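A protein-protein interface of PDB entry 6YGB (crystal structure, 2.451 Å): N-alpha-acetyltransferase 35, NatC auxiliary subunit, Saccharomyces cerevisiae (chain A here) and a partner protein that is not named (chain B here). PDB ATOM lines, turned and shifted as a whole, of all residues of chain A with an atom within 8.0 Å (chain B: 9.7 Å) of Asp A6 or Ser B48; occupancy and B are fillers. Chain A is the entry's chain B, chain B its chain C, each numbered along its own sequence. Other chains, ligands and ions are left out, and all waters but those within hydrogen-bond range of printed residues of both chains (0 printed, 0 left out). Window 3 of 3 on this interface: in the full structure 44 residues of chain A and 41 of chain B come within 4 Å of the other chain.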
ATOM      1  N   PRO A   2      27.755  -1.387 -17.788  1.00  0.00           N
ATOM      2  CA  PRO A   2      26.773  -1.116 -18.847  1.00  0.00           C
ATOM      3  C   PRO A   2      26.116   0.251 -18.676  1.00  0.00           C
ATOM      4  O   PRO A   2      26.198   0.812 -17.587  1.00  0.00           O
ATOM      5  CB  PRO A   2      25.747  -2.244 -18.673  1.00  0.00           C
ATOM      6  CG  PRO A   2      26.462  -3.306 -17.882  1.00  0.00           C
ATOM      7  CD  PRO A   2      27.379  -2.554 -16.973  1.00  0.00           C
ATOM      8  N   MET A   3      25.476   0.776 -19.727  1.00  0.00           N
ATOM      9  CA  MET A   3      24.836   2.089 -19.637  1.00  0.00           C
ATOM     10  C   MET A   3      23.691   2.119 -18.630  1.00  0.00           C
ATOM     11  O   MET A   3      23.343   3.200 -18.141  1.00  0.00           O
ATOM     12  CB  MET A   3      24.329   2.532 -21.018  1.00  0.00           C
ATOM     13  CG  MET A   3      25.331   3.352 -21.834  1.00  0.00           C
ATOM     14  SD  MET A   3      24.604   4.324 -23.185  1.00  0.00           S
ATOM     15  CE  MET A   3      23.489   5.410 -22.302  1.00  0.00           C
ATOM     16  N   GLU A   4      23.117   0.967 -18.298  1.00  0.00           N
ATOM     17  CA  GLU A   4      21.987   0.920 -17.381  1.00  0.00           C
ATOM     18  C   GLU A   4      22.423   1.268 -15.960  1.00  0.00           C
ATOM     19  O   GLU A   4      23.558   1.007 -15.550  1.00  0.00           O
ATOM     20  CB  GLU A   4      21.343  -0.466 -17.396  1.00  0.00           C
ATOM     21  CG  GLU A   4      19.927  -0.501 -16.846  1.00  0.00           C
ATOM     22  CD  GLU A   4      19.389  -1.912 -16.732  1.00  0.00           C
ATOM     23  OE1 GLU A   4      20.152  -2.794 -16.289  1.00  0.00           O
ATOM     24  OE2 GLU A   4      18.214  -2.144 -17.097  1.00  0.00           O
ATOM     25  N   VAL A   5      21.489   1.837 -15.195  1.00  0.00           N
ATOM     26  CA  VAL A   5      21.813   2.379 -13.875  1.00  0.00           C
ATOM     27  C   VAL A   5      22.096   1.261 -12.875  1.00  0.00           C
ATOM     28  O   VAL A   5      23.125   1.269 -12.188  1.00  0.00           O
ATOM     29  CB  VAL A   5      20.677   3.293 -13.382  1.00  0.00           C
ATOM     30  CG1 VAL A   5      21.169   4.196 -12.260  1.00  0.00           C
ATOM     31  CG2 VAL A   5      20.120   4.109 -14.538  1.00  0.00           C
ATOM     32  N   ASP A   6      21.178   0.295 -12.755  1.00  0.00           N
ATOM     33  CA  ASP A   6      21.340  -0.744 -11.740  1.00  0.00           C
ATOM     34  C   ASP A   6      22.560  -1.617 -12.000  1.00  0.00           C
ATOM     35  O   ASP A   6      23.143  -2.161 -11.056  1.00  0.00           O
ATOM     36  CB  ASP A   6      20.082  -1.605 -11.650  1.00  0.00           C
ATOM     37  CG  ASP A   6      18.974  -0.929 -10.863  1.00  0.00           C
ATOM     38  OD1 ASP A   6      19.033   0.308 -10.692  1.00  0.00           O
ATOM     39  OD2 ASP A   6      18.050  -1.637 -10.406  1.00  0.00           O
ATOM     40  N   SER A   7      22.966  -1.760 -13.262  1.00  0.00           N
ATOM     41  CA  SER A   7      24.166  -2.536 -13.555  1.00  0.00           C
ATOM     42  C   SER A   7      25.411  -1.825 -13.041  1.00  0.00           C
ATOM     43  O   SER A   7      26.323  -2.462 -12.503  1.00  0.00           O
ATOM     44  CB  SER A   7      24.267  -2.799 -15.058  1.00  0.00           C
ATOM     45  OG  SER A   7      24.232  -1.590 -15.799  1.00  0.00           O
ATOM     46  N   ILE A   8      25.456  -0.499 -13.189  1.00  0.00           N
ATOM     47  CA  ILE A   8      26.584   0.284 -12.689  1.00  0.00           C
ATOM     48  C   ILE A   8      26.688   0.165 -11.174  1.00  0.00           C
ATOM     49  O   ILE A   8      27.754  -0.138 -10.627  1.00  0.00           O
ATOM     50  CB  ILE A   8      26.444   1.752 -13.127  1.00  0.00           C
ATOM     51  CG1 ILE A   8      26.604   1.868 -14.644  1.00  0.00           C
ATOM     52  CG2 ILE A   8      27.445   2.630 -12.399  1.00  0.00           C
ATOM     53  CD1 ILE A   8      26.302   3.244 -15.182  1.00  0.00           C
ATOM     54  N   LEU A   9      25.576   0.396 -10.475  1.00  0.00           N
ATOM     55  CA  LEU A   9      25.595   0.389  -9.016  1.00  0.00           C
ATOM     56  C   LEU A   9      25.794  -1.012  -8.453  1.00  0.00           C
ATOM     57  O   LEU A   9      26.415  -1.170  -7.393  1.00  0.00           O
ATOM     58  CB  LEU A   9      24.303   1.011  -8.481  1.00  0.00           C
ATOM     59  CG  LEU A   9      24.109   2.491  -8.809  1.00  0.00           C
ATOM     60  CD1 LEU A   9      22.731   2.962  -8.377  1.00  0.00           C
ATOM     61  CD2 LEU A   9      25.192   3.321  -8.147  1.00  0.00           C
ATOM     62  N   GLY A  10      25.291  -2.038  -9.147  1.00  0.00           N
ATOM     63  CA  GLY A  10      25.433  -3.398  -8.653  1.00  0.00           C
ATOM     64  C   GLY A  10      26.870  -3.873  -8.596  1.00  0.00           C
ATOM     65  O   GLY A  10      27.212  -4.730  -7.776  1.00  0.00           O
ATOM     66  N   SER A  11      27.727  -3.322  -9.454  1.00  0.00           N
ATOM     67  CA  SER A  11      29.128  -3.728  -9.472  1.00  0.00           C
ATOM     68  C   SER A  11      29.834  -3.393  -8.163  1.00  0.00           C
ATOM     69  O   SER A  11      30.736  -4.125  -7.735  1.00  0.00           O
ATOM     70  CB  SER A  11      29.853  -3.074 -10.649  1.00  0.00           C
ATOM     71  OG  SER A  11      29.314  -3.503 -11.890  1.00  0.00           O
ATOM     72  N   LEU A  12      29.442  -2.298  -7.513  1.00  0.00           N
ATOM     73  CA  LEU A  12      30.064  -1.940  -6.244  1.00  0.00           C
ATOM     74  C   LEU A  12      29.724  -2.935  -5.144  1.00  0.00           C
ATOM     75  O   LEU A  12      30.532  -3.146  -4.230  1.00  0.00           O
ATOM     76  CB  LEU A  12      29.630  -0.541  -5.816  1.00  0.00           C
ATOM     77  CG  LEU A  12      29.955   0.611  -6.762  1.00  0.00           C
ATOM     78  CD1 LEU A  12      29.389   1.906  -6.208  1.00  0.00           C
ATOM     79  CD2 LEU A  12      31.453   0.720  -6.960  1.00  0.00           C
ATOM     80  N   ILE A  14      29.020  -6.237  -5.470  1.00  0.00           N
ATOM     81  CA  ILE A  14      29.192  -7.642  -5.834  1.00  0.00           C
ATOM     82  C   ILE A  14      29.862  -8.415  -4.707  1.00  0.00           C
ATOM     83  O   ILE A  14      29.435  -9.521  -4.353  1.00  0.00           O
ATOM     84  CB  ILE A  14      29.994  -7.763  -7.142  1.00  0.00           C
ATOM     85  CG1 ILE A  14      29.230  -7.120  -8.299  1.00  0.00           C
ATOM     86  CG2 ILE A  14      30.300  -9.219  -7.443  1.00  0.00           C
ATOM     87  CD1 ILE A  14      29.922  -7.256  -9.635  1.00  0.00           C
ATOM     88  N   ASP B  21      33.955  -8.734 -17.384  1.00  0.00           N
ATOM     89  CA  ASP B  21      33.490  -8.310 -16.059  1.00  0.00           C
ATOM     90  C   ASP B  21      32.370  -9.225 -15.555  1.00  0.00           C
ATOM     91  O   ASP B  21      31.242  -8.811 -15.294  1.00  0.00           O
ATOM     92  CB  ASP B  21      33.072  -6.840 -16.073  1.00  0.00           C
ATOM     93  CG  ASP B  21      31.971  -6.543 -17.075  1.00  0.00           C
ATOM     94  OD1 ASP B  21      31.500  -7.487 -17.749  1.00  0.00           O
ATOM     95  OD2 ASP B  21      31.579  -5.363 -17.191  1.00  0.00           O
ATOM     96  N   ARG B  22      32.712 -10.506 -15.430  1.00  0.00           N
ATOM     97  CA  ARG B  22      31.848 -11.503 -14.821  1.00  0.00           C
ATOM     98  C   ARG B  22      32.644 -12.220 -13.745  1.00  0.00           C
ATOM     99  O   ARG B  22      33.844 -12.457 -13.909  1.00  0.00           O
ATOM    100  CB  ARG B  22      31.316 -12.507 -15.862  1.00  0.00           C
ATOM    101  CG  ARG B  22      32.401 -13.220 -16.652  1.00  0.00           C
ATOM    102  CD  ARG B  22      31.854 -13.977 -17.859  1.00  0.00           C
ATOM    103  NE  ARG B  22      31.080 -15.161 -17.497  1.00  0.00           N
ATOM    104  CZ  ARG B  22      30.963 -16.237 -18.271  1.00  0.00           C
ATOM    105  NH1 ARG B  22      31.581 -16.287 -19.444  1.00  0.00           N
ATOM    106  NH2 ARG B  22      30.236 -17.271 -17.869  1.00  0.00           N
ATOM    107  N   GLU B  43      28.056 -19.626  -9.006  1.00  0.00           N
ATOM    108  CA  GLU B  43      27.169 -18.489  -9.196  1.00  0.00           C
ATOM    109  C   GLU B  43      27.891 -17.489 -10.081  1.00  0.00           C
ATOM    110  O   GLU B  43      28.985 -17.035  -9.733  1.00  0.00           O
ATOM    111  CB  GLU B  43      26.793 -17.850  -7.862  1.00  0.00           C
ATOM    112  CG  GLU B  43      25.711 -16.794  -7.967  1.00  0.00           C
ATOM    113  CD  GLU B  43      25.600 -15.945  -6.715  1.00  0.00           C
ATOM    114  OE1 GLU B  43      26.374 -16.173  -5.762  1.00  0.00           O
ATOM    115  OE2 GLU B  43      24.740 -15.040  -6.684  1.00  0.00           O
ATOM    116  N   GLU B  44      27.292 -17.161 -11.220  1.00  0.00           N
ATOM    117  CA  GLU B  44      27.851 -16.184 -12.144  1.00  0.00           C
ATOM    118  C   GLU B  44      27.249 -14.818 -11.839  1.00  0.00           C
ATOM    119  O   GLU B  44      26.025 -14.648 -11.903  1.00  0.00           O
ATOM    120  CB  GLU B  44      27.572 -16.573 -13.595  1.00  0.00           C
ATOM    121  CG  GLU B  44      28.300 -15.703 -14.607  1.00  0.00           C
ATOM    122  CD  GLU B  44      27.512 -15.498 -15.888  1.00  0.00           C
ATOM    123  OE1 GLU B  44      26.275 -15.345 -15.814  1.00  0.00           O
ATOM    124  OE2 GLU B  44      28.135 -15.489 -16.969  1.00  0.00           O
ATOM    125  N   ARG B  45      28.105 -13.847 -11.524  1.00  0.00           N
ATOM    126  CA  ARG B  45      27.675 -12.491 -11.199  1.00  0.00           C
ATOM    127  C   ARG B  45      28.218 -11.521 -12.239  1.00  0.00           C
ATOM    128  O   ARG B  45      29.435 -11.427 -12.433  1.00  0.00           O
ATOM    129  CB  ARG B  45      28.134 -12.096  -9.793  1.00  0.00           C
ATOM    130  CG  ARG B  45      27.492 -12.917  -8.683  1.00  0.00           C
ATOM    131  CD  ARG B  45      28.049 -12.574  -7.308  1.00  0.00           C
ATOM    132  NE  ARG B  45      27.366 -13.339  -6.269  1.00  0.00           N
ATOM    133  CZ  ARG B  45      27.680 -13.315  -4.977  1.00  0.00           C
ATOM    134  NH1 ARG B  45      28.679 -12.559  -4.544  1.00  0.00           N
ATOM    135  NH2 ARG B  45      26.991 -14.052  -4.118  1.00  0.00           N
ATOM    136  N   MET B  46      27.313 -10.800 -12.901  1.00  0.00           N
ATOM    137  CA  MET B  46      27.665  -9.773 -13.883  1.00  0.00           C
ATOM    138  C   MET B  46      26.878  -8.511 -13.551  1.00  0.00           C
ATOM    139  O   MET B  46      25.685  -8.429 -13.851  1.00  0.00           O
ATOM    140  CB  MET B  46      27.364 -10.231 -15.307  1.00  0.00           C
ATOM    141  CG  MET B  46      27.939 -11.581 -15.676  1.00  0.00           C
ATOM    142  SD  MET B  46      27.805 -11.903 -17.445  1.00  0.00           S
ATOM    143  CE  MET B  46      28.731 -10.518 -18.104  1.00  0.00           C
ATOM    144  N   GLY B  47      27.547  -7.538 -12.948  1.00  0.00           N
ATOM    145  CA  GLY B  47      26.902  -6.271 -12.651  1.00  0.00           C
ATOM    146  C   GLY B  47      25.764  -6.443 -11.665  1.00  0.00           C
ATOM    147  O   GLY B  47      25.968  -6.790 -10.493  1.00  0.00           O
ATOM    148  N   SER B  48      24.541  -6.182 -12.135  1.00  0.00           N
ATOM    149  CA  SER B  48      23.373  -6.337 -11.275  1.00  0.00           C
ATOM    150  C   SER B  48      22.933  -7.793 -11.186  1.00  0.00           C
ATOM    151  O   SER B  48      22.436  -8.233 -10.143  1.00  0.00           O
ATOM    152  CB  SER B  48      22.224  -5.471 -11.789  1.00  0.00           C
ATOM    153  OG  SER B  48      21.937  -5.762 -13.146  1.00  0.00           O
ATOM    154  N   SER B  49      23.114  -8.556 -12.261  1.00  0.00           N
ATOM    155  CA  SER B  49      22.493  -9.864 -12.391  1.00  0.00           C
ATOM    156  C   SER B  49      23.293 -10.962 -11.686  1.00  0.00           C
ATOM    157  O   SER B  49      24.505 -10.868 -11.473  1.00  0.00           O
ATOM    158  CB  SER B  49      22.320 -10.230 -13.865  1.00  0.00           C
ATOM    159  OG  SER B  49      21.309  -9.444 -14.474  1.00  0.00           O
ATOM    160  N   SER B  50      22.577 -12.030 -11.342  1.00  0.00           N
ATOM    161  CA  SER B  50      23.134 -13.216 -10.712  1.00  0.00           C
ATOM    162  C   SER B  50      22.409 -14.440 -11.249  1.00  0.00           C
ATOM    163  O   SER B  50      21.205 -14.385 -11.512  1.00  0.00           O
ATOM    164  CB  SER B  50      23.003 -13.143  -9.185  1.00  0.00           C
ATOM    165  OG  SER B  50      23.228 -14.402  -8.581  1.00  0.00           O
ATOM    166  N   ARG B  51      23.142 -15.541 -11.415  1.00  0.00           N
ATOM    167  CA  ARG B  51      22.535 -16.782 -11.882  1.00  0.00           C
ATOM    168  C   ARG B  51      23.432 -17.955 -11.515  1.00  0.00           C
ATOM    169  O   ARG B  51      24.627 -17.796 -11.261  1.00  0.00           O
ATOM    170  CB  ARG B  51      22.278 -16.756 -13.393  1.00  0.00           C
ATOM    171  CG  ARG B  51      23.519 -16.853 -14.262  1.00  0.00           C
ATOM    172  CD  ARG B  51      23.118 -17.103 -15.706  1.00  0.00           C
ATOM    173  NE  ARG B  51      24.263 -17.287 -16.592  1.00  0.00           N
ATOM    174  CZ  ARG B  51      24.187 -17.846 -17.794  1.00  0.00           C
ATOM    175  NH1 ARG B  51      23.020 -18.285 -18.247  1.00  0.00           N
ATOM    176  NH2 ARG B  51      25.275 -17.975 -18.543  1.00  0.00           N
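O of Ile A14 is in hydrogen-bond range of NH1 of Arg B45, 3.1 Å away.
The backbone carbonyl oxygen (O) of Ser A7 sits at hydrogen-bond distance from the side-chain hydroxyl (OG) of Ser A11 (3.2 Å). O of Glu A4 is in hydrogen-bond range of OG of Ser A7 (2.7 Å). The guanidinium group of Arg B45 is in salt-bridge range of the side-chain carboxylate of Glu B43, 2.8 Å away.
Asp A6 touches Ser B48 (O to CB, 3.5 Å). Ser A7 touches Gly B47. Ser B48 touches Ser A7. O of Gly B47 touches C of Gly A10, 3.6 Å away. Ser A11 touches Gly B47. CG1 of Ile A14 touches O of Gly B47, at 3.9 Å.
Asp A6 touches just one residue of chain B: Ser B48 (3.5 Å). Ser B48 touches just these residues of chain A: Asp A6 (3.5 Å) and Ser A7 (3.9 Å). No residue of chain B comes within 4 Å of Val A5. Of chain B, only Gly B47 (3.9 Å) and Ser B48 (3.9 Å) come within 4 Å of Ser A7. Gly A10 touches just one residue of chain B: Gly B47. Printed residues of chain B within 4 Å of Ser A11: Gly B47. Printed residues of chain B within 4 Å of Ile A14: Arg B45 (3.1 Å) and Gly B47 (3.9 Å). Of the printed residues of chain A, Arg B45 touches Ile A14 (3.1 Å). The nearest residue of chain A that does not touch Ser B48 is Gly A10 (4.4 Å).
Hydrophobic or aromatic side chains of chain A within 4 Å of the printed part of chain B: Ile A14. Among the printed residues, 7 pairs touch across the chains. Among the printed residues, no Asp or Glu carboxylate lies within 4 Å of a Lys or Arg side-chain nitrogen of the other chain.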
